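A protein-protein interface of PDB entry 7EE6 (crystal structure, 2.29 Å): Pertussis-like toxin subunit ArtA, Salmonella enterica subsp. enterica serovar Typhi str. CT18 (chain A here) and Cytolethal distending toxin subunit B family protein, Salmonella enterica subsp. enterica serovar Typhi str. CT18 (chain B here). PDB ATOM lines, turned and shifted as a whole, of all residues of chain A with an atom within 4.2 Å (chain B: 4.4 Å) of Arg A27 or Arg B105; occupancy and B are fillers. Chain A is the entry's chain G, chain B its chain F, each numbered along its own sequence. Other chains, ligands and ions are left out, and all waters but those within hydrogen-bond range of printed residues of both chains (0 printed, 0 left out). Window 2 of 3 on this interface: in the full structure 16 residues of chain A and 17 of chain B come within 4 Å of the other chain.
Arg A27 touches just these residues of chain B: Thr B34, Asp B38 and Arg B105.
Arg B105 touches just these residues of chain A: Arg A27 and Phe A167.
Of the printed residues of chain A, Thr B34 touches Arg A27 (2.5 Å) and Phe A167 (3.4 Å).
Printed residues of chain A within 4 Å of Gln B106: Phe A167 (3.6 Å).
Of the printed residues of chain B, Phe A167 touches Thr B34, Arg B105 and Gln B106.
Of the printed residues of chain A, Asp B38 touches Arg A27 and Arg A46.
Arg B84 touches none of the printed residues of chain A.
The nearest printed residue of chain B that does not touch Arg A27 is Gly B36 (4.9 Å).
The nearest printed residue of chain A that does not touch Arg B105 is Arg A46 (6.2 Å).
The nearest printed residue of chain A that does not touch Thr B34 is Pro A169 (4.004 Å).
The backbone carbonyl oxygen (O) of Thr B34 is in hydrogen-bond range of the guanidinium group (NH1) of Arg A27 (2.5 Å).
The guanidinium group (NH2) of Arg A27 is in salt-bridge range of the side-chain carboxylate (OD1) of Asp B38 (3.5 Å).
The side-chain carboxylate of Asp B38 is in salt-bridge range of the guanidinium group of Arg A46.
NH2 of Arg B105 touches NH1 of Arg A27, 3.9 Å away.
Phe A167 touches Thr B34 (O to CG2, 3.4 Å).
Phe A167 touches Arg B105 (CE1 to CD, 3.7 Å).
CZ of Phe A167 touches CG of Gln B106, at 3.6 Å.
Of the 11 printed residues of chain B, 4 touch a printed residue of chain A.
Of the 9 printed residues of chain A, 3 touch a printed residue of chain B.
Printed residues of chain A that touch a printed residue of chain B: Arg A27, Arg A46 and Phe A167.
Hydrophobic or aromatic side chains of chain A within 4 Å of the printed part of chain B: Phe A167.
O of Gly B33 sits at hydrogen-bond distance from NH2 of Arg B105, at 2.8 Å.
The backbone carbonyl oxygen (O) of Thr B34 sits at hydrogen-bond distance from the guanidinium group (NH2) of Arg B105 (3.2 Å).
NE of Arg B105 is in salt-bridge range of OD1 of Asp B38 (2.8 Å).
O of Gln B106 lies within hydrogen-bond range of OG of Ser B104 (2.7 Å).
The backbone NH (N) of Arg A46 is in hydrogen-bond range of the backbone carbonyl oxygen (O) of Asn A26 (3.0 Å).
The backbone carbonyl oxygen (O) of Arg A27 sits at hydrogen-bond distance from the side-chain hydroxyl (OH) of Tyr A47 (2.6 Å).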
ATOM      1  N   TYR A  25       9.974  -3.485  -3.110  1.00  0.00           N
ATOM      2  CA  TYR A  25      11.207  -2.953  -3.671  1.00  0.00           C
ATOM      3  C   TYR A  25      11.627  -1.613  -3.055  1.00  0.00           C
ATOM      4  O   TYR A  25      12.612  -1.017  -3.509  1.00  0.00           O
ATOM      5  CB  TYR A  25      11.052  -2.814  -5.190  1.00  0.00           C
ATOM      6  CG  TYR A  25      10.980  -4.134  -5.945  1.00  0.00           C
ATOM      7  CD1 TYR A  25      12.068  -5.006  -5.950  1.00  0.00           C
ATOM      8  CD2 TYR A  25       9.851  -4.490  -6.682  1.00  0.00           C
ATOM      9  CE1 TYR A  25      12.031  -6.201  -6.633  1.00  0.00           C
ATOM     10  CE2 TYR A  25       9.802  -5.699  -7.393  1.00  0.00           C
ATOM     11  CZ  TYR A  25      10.904  -6.548  -7.361  1.00  0.00           C
ATOM     12  OH  TYR A  25      10.912  -7.746  -8.045  1.00  0.00           O
ATOM     13  N   ASN A  26      10.918  -1.129  -2.033  1.00  0.00           N
ATOM     14  CA  ASN A  26      11.144   0.222  -1.512  1.00  0.00           C
ATOM     15  C   ASN A  26      12.432   0.275  -0.691  1.00  0.00           C
ATOM     16  O   ASN A  26      12.464  -0.146   0.467  1.00  0.00           O
ATOM     17  CB  ASN A  26       9.952   0.675  -0.677  1.00  0.00           C
ATOM     18  CG  ASN A  26      10.014   2.168  -0.316  1.00  0.00           C
ATOM     19  OD1 ASN A  26      11.032   2.833  -0.511  1.00  0.00           O
ATOM     20  ND2 ASN A  26       8.936   2.673   0.245  1.00  0.00           N
ATOM     21  N   ARG A  27      13.475   0.847  -1.279  1.00  0.00           N
ATOM     22  CA  ARG A  27      14.790   0.975  -0.672  1.00  0.00           C
ATOM     23  C   ARG A  27      14.926   2.175   0.267  1.00  0.00           C
ATOM     24  O   ARG A  27      15.975   2.302   0.916  1.00  0.00           O
ATOM     25  CB  ARG A  27      15.854   1.081  -1.777  1.00  0.00           C
ATOM     26  CG  ARG A  27      16.032  -0.170  -2.641  1.00  0.00           C
ATOM     27  CD  ARG A  27      17.178   0.014  -3.632  1.00  0.00           C
ATOM     28  NE  ARG A  27      17.851  -1.259  -3.914  1.00  0.00           N
ATOM     29  CZ  ARG A  27      17.989  -1.773  -5.130  1.00  0.00           C
ATOM     30  NH1 ARG A  27      17.524  -1.115  -6.174  1.00  0.00           N
ATOM     31  NH2 ARG A  27      18.607  -2.928  -5.314  1.00  0.00           N
ATOM     32  N   ASN A  28      13.918   3.057   0.350  1.00  0.00           N
ATOM     33  CA  ASN A  28      14.046   4.294   1.133  1.00  0.00           C
ATOM     34  C   ASN A  28      14.341   3.998   2.603  1.00  0.00           C
ATOM     35  O   ASN A  28      13.507   3.415   3.307  1.00  0.00           O
ATOM     36  CB  ASN A  28      12.771   5.131   1.020  1.00  0.00           C
ATOM     37  CG  ASN A  28      12.883   6.482   1.736  1.00  0.00           C
ATOM     38  OD1 ASN A  28      13.133   6.544   2.951  1.00  0.00           O
ATOM     39  ND2 ASN A  28      12.645   7.559   1.001  1.00  0.00           N
ATOM     40  N   PHE A  29      15.503   4.462   3.084  1.00  0.00           N
ATOM     41  CA  PHE A  29      15.941   4.079   4.428  1.00  0.00           C
ATOM     42  C   PHE A  29      15.066   4.699   5.521  1.00  0.00           C
ATOM     43  O   PHE A  29      14.682   4.008   6.473  1.00  0.00           O
ATOM     44  CB  PHE A  29      17.407   4.447   4.640  1.00  0.00           C
ATOM     45  CG  PHE A  29      17.974   4.014   5.986  1.00  0.00           C
ATOM     46  CD1 PHE A  29      18.510   2.743   6.160  1.00  0.00           C
ATOM     47  CD2 PHE A  29      17.974   4.883   7.070  1.00  0.00           C
ATOM     48  CE1 PHE A  29      19.042   2.341   7.376  1.00  0.00           C
ATOM     49  CE2 PHE A  29      18.510   4.494   8.305  1.00  0.00           C
ATOM     50  CZ  PHE A  29      19.043   3.218   8.454  1.00  0.00           C
ATOM     51  N   ARG A  46      11.896  -3.029   0.982  1.00  0.00           N
ATOM     52  CA  ARG A  46      12.901  -3.955   0.472  1.00  0.00           C
ATOM     53  C   ARG A  46      13.865  -4.417   1.564  1.00  0.00           C
ATOM     54  O   ARG A  46      15.047  -4.666   1.290  1.00  0.00           O
ATOM     55  CB  ARG A  46      13.665  -3.300  -0.682  1.00  0.00           C
ATOM     56  CG  ARG A  46      14.221  -4.273  -1.708  1.00  0.00           C
ATOM     57  CD  ARG A  46      14.780  -3.514  -2.889  1.00  0.00           C
ATOM     58  NE  ARG A  46      15.277  -4.397  -3.931  1.00  0.00           N
ATOM     59  CZ  ARG A  46      15.342  -4.058  -5.219  1.00  0.00           C
ATOM     60  NH1 ARG A  46      14.928  -2.859  -5.621  1.00  0.00           N
ATOM     61  NH2 ARG A  46      15.810  -4.922  -6.099  1.00  0.00           N
ATOM     62  N   TYR A  47      13.390  -4.515   2.804  1.00  0.00           N
ATOM     63  CA  TYR A  47      14.222  -4.901   3.933  1.00  0.00           C
ATOM     64  C   TYR A  47      13.397  -5.762   4.870  1.00  0.00           C
ATOM     65  O   TYR A  47      12.173  -5.645   4.923  1.00  0.00           O
ATOM     66  CB  TYR A  47      14.770  -3.680   4.717  1.00  0.00           C
ATOM     67  CG  TYR A  47      15.467  -2.623   3.869  1.00  0.00           C
ATOM     68  CD1 TYR A  47      16.737  -2.846   3.350  1.00  0.00           C
ATOM     69  CD2 TYR A  47      14.872  -1.402   3.612  1.00  0.00           C
ATOM     70  CE1 TYR A  47      17.386  -1.891   2.579  1.00  0.00           C
ATOM     71  CE2 TYR A  47      15.521  -0.435   2.851  1.00  0.00           C
ATOM     72  CZ  TYR A  47      16.772  -0.693   2.337  1.00  0.00           C
ATOM     73  OH  TYR A  47      17.416   0.259   1.569  1.00  0.00           O
ATOM     74  N   PHE A 167      23.235   0.782  -2.412  1.00  0.00           N
ATOM     75  CA  PHE A 167      22.150   1.262  -3.275  1.00  0.00           C
ATOM     76  C   PHE A 167      21.143   2.093  -2.506  1.00  0.00           C
ATOM     77  O   PHE A 167      19.969   2.165  -2.882  1.00  0.00           O
ATOM     78  CB  PHE A 167      21.436   0.106  -3.998  1.00  0.00           C
ATOM     79  CG  PHE A 167      22.360  -0.976  -4.440  1.00  0.00           C
ATOM     80  CD1 PHE A 167      23.475  -0.668  -5.210  1.00  0.00           C
ATOM     81  CD2 PHE A 167      22.141  -2.295  -4.078  1.00  0.00           C
ATOM     82  CE1 PHE A 167      24.341  -1.662  -5.621  1.00  0.00           C
ATOM     83  CE2 PHE A 167      23.007  -3.291  -4.488  1.00  0.00           C
ATOM     84  CZ  PHE A 167      24.106  -2.973  -5.259  1.00  0.00           C
ATOM     85  N   PRO A 169      18.886   4.937  -1.536  1.00  0.00           N
ATOM     86  CA  PRO A 169      18.401   6.152  -2.186  1.00  0.00           C
ATOM     87  C   PRO A 169      18.952   7.384  -1.487  1.00  0.00           C
ATOM     88  O   PRO A 169      19.195   7.390  -0.271  1.00  0.00           O
ATOM     89  CB  PRO A 169      16.878   6.058  -2.040  1.00  0.00           C
ATOM     90  CG  PRO A 169      16.603   4.631  -1.787  1.00  0.00           C
ATOM     91  CD  PRO A 169      17.784   4.102  -1.043  1.00  0.00           C
ATOM     92  N   LEU B  31      17.912   0.804 -16.614  1.00  0.00           N
ATOM     93  CA  LEU B  31      18.685   0.493 -15.418  1.00  0.00           C
ATOM     94  C   LEU B  31      18.857   1.661 -14.452  1.00  0.00           C
ATOM     95  O   LEU B  31      19.125   1.415 -13.268  1.00  0.00           O
ATOM     96  CB  LEU B  31      20.078  -0.027 -15.799  1.00  0.00           C
ATOM     97  CG  LEU B  31      20.092  -1.244 -16.719  1.00  0.00           C
ATOM     98  CD1 LEU B  31      21.500  -1.574 -17.143  1.00  0.00           C
ATOM     99  CD2 LEU B  31      19.466  -2.412 -16.015  1.00  0.00           C
ATOM    100  N   GLY B  33      19.032   4.701 -11.797  1.00  0.00           N
ATOM    101  CA  GLY B  33      18.429   4.951 -10.508  1.00  0.00           C
ATOM    102  C   GLY B  33      18.467   3.730  -9.604  1.00  0.00           C
ATOM    103  O   GLY B  33      18.782   2.607 -10.016  1.00  0.00           O
ATOM    104  N   THR B  34      18.147   3.971  -8.326  1.00  0.00           N
ATOM    105  CA  THR B  34      17.991   2.866  -7.387  1.00  0.00           C
ATOM    106  C   THR B  34      16.762   2.033  -7.723  1.00  0.00           C
ATOM    107  O   THR B  34      16.763   0.822  -7.500  1.00  0.00           O
ATOM    108  CB  THR B  34      17.906   3.382  -5.941  1.00  0.00           C
ATOM    109  OG1 THR B  34      16.806   4.292  -5.806  1.00  0.00           O
ATOM    110  CG2 THR B  34      19.200   4.086  -5.521  1.00  0.00           C
ATOM    111  N   GLY B  36      15.877   1.406 -10.746  1.00  0.00           N
ATOM    112  CA  GLY B  36      16.099   0.792 -12.042  1.00  0.00           C
ATOM    113  C   GLY B  36      16.153  -0.732 -11.973  1.00  0.00           C
ATOM    114  O   GLY B  36      16.141  -1.353 -10.904  1.00  0.00           O
ATOM    115  N   VAL B  37      16.193  -1.348 -13.159  1.00  0.00           N
ATOM    116  CA  VAL B  37      16.261  -2.804 -13.261  1.00  0.00           C
ATOM    117  C   VAL B  37      17.593  -3.291 -12.702  1.00  0.00           C
ATOM    118  O   VAL B  37      18.655  -2.719 -12.989  1.00  0.00           O
ATOM    119  CB  VAL B  37      16.068  -3.250 -14.722  1.00  0.00           C
ATOM    120  CG1 VAL B  37      16.494  -4.687 -14.897  1.00  0.00           C
ATOM    121  CG2 VAL B  37      14.626  -3.066 -15.158  1.00  0.00           C
ATOM    122  N   ASP B  38      17.548  -4.351 -11.898  1.00  0.00           N
ATOM    123  CA  ASP B  38      18.749  -4.886 -11.263  1.00  0.00           C
ATOM    124  C   ASP B  38      19.473  -5.883 -12.142  1.00  0.00           C
ATOM    125  O   ASP B  38      20.711  -5.915 -12.164  1.00  0.00           O
ATOM    126  CB  ASP B  38      18.381  -5.556  -9.937  1.00  0.00           C
ATOM    127  CG  ASP B  38      17.690  -4.603  -8.996  1.00  0.00           C
ATOM    128  OD1 ASP B  38      18.291  -3.535  -8.731  1.00  0.00           O
ATOM    129  OD2 ASP B  38      16.548  -4.892  -8.558  1.00  0.00           O
ATOM    130  N   ILE B  83      28.059   2.110 -10.868  1.00  0.00           N
ATOM    131  CA  ILE B  83      28.767   1.069 -11.612  1.00  0.00           C
ATOM    132  C   ILE B  83      27.874  -0.162 -11.736  1.00  0.00           C
ATOM    133  O   ILE B  83      27.443  -0.730 -10.725  1.00  0.00           O
ATOM    134  CB  ILE B  83      30.105   0.717 -10.935  1.00  0.00           C
ATOM    135  CG1 ILE B  83      31.044   1.928 -10.918  1.00  0.00           C
ATOM    136  CG2 ILE B  83      30.793  -0.425 -11.643  1.00  0.00           C
ATOM    137  CD1 ILE B  83      31.157   2.645 -12.257  1.00  0.00           C
ATOM    138  N   ARG B  84      27.589  -0.562 -12.976  1.00  0.00           N
ATOM    139  CA  ARG B  84      26.932  -1.824 -13.287  1.00  0.00           C
ATOM    140  C   ARG B  84      27.934  -2.751 -13.958  1.00  0.00           C
ATOM    141  O   ARG B  84      28.888  -2.300 -14.597  1.00  0.00           O
ATOM    142  CB  ARG B  84      25.721  -1.627 -14.203  1.00  0.00           C
ATOM    143  CG  ARG B  84      24.794  -0.501 -13.801  1.00  0.00           C
ATOM    144  CD  ARG B  84      24.191  -0.737 -12.426  1.00  0.00           C
ATOM    145  NE  ARG B  84      23.404   0.409 -11.997  1.00  0.00           N
ATOM    146  CZ  ARG B  84      22.087   0.515 -12.137  1.00  0.00           C
ATOM    147  NH1 ARG B  84      21.396  -0.473 -12.690  1.00  0.00           N
ATOM    148  NH2 ARG B  84      21.463   1.613 -11.725  1.00  0.00           N
ATOM    149  N   SER B 104      24.257  -6.524 -14.469  1.00  0.00           N
ATOM    150  CA  SER B 104      23.981  -6.743 -13.061  1.00  0.00           C
ATOM    151  C   SER B 104      24.415  -5.526 -12.253  1.00  0.00           C
ATOM    152  O   SER B 104      25.419  -4.876 -12.559  1.00  0.00           O
ATOM    153  CB  SER B 104      24.696  -8.003 -12.538  1.00  0.00           C
ATOM    154  OG  SER B 104      24.571  -8.110 -11.122  1.00  0.00           O
ATOM    155  N   ARG B 105      23.645  -5.230 -11.211  1.00  0.00           N
ATOM    156  CA  ARG B 105      23.992  -4.152 -10.300  1.00  0.00           C
ATOM    157  C   ARG B 105      25.170  -4.499  -9.390  1.00  0.00           C
ATOM    158  O   ARG B 105      25.748  -3.591  -8.788  1.00  0.00           O
ATOM    159  CB  ARG B 105      22.767  -3.786  -9.467  1.00  0.00           C
ATOM    160  CG  ARG B 105      22.781  -2.384  -8.962  1.00  0.00           C
ATOM    161  CD  ARG B 105      21.616  -2.120  -8.038  1.00  0.00           C
ATOM    162  NE  ARG B 105      20.382  -1.741  -8.730  1.00  0.00           N
ATOM    163  CZ  ARG B 105      20.075  -0.489  -9.082  1.00  0.00           C
ATOM    164  NH1 ARG B 105      20.942   0.494  -8.850  1.00  0.00           N
ATOM    165  NH2 ARG B 105      18.914  -0.214  -9.680  1.00  0.00           N
ATOM    166  N   GLN B 106      25.534  -5.778  -9.292  1.00  0.00           N
ATOM    167  CA  GLN B 106      26.597  -6.263  -8.422  1.00  0.00           C
ATOM    168  C   GLN B 106      27.510  -7.227  -9.180  1.00  0.00           C
ATOM    169  O   GLN B 106      27.091  -7.901 -10.124  1.00  0.00           O
ATOM    170  CB  GLN B 106      26.035  -6.973  -7.186  1.00  0.00           C
ATOM    171  CG  GLN B 106      24.903  -6.237  -6.506  1.00  0.00           C
ATOM    172  CD  GLN B 106      24.312  -7.027  -5.344  1.00  0.00           C
ATOM    173  OE1 GLN B 106      23.090  -7.139  -5.208  1.00  0.00           O
ATOM    174  NE2 GLN B 106      25.183  -7.573  -4.494  1.00  0.00           N
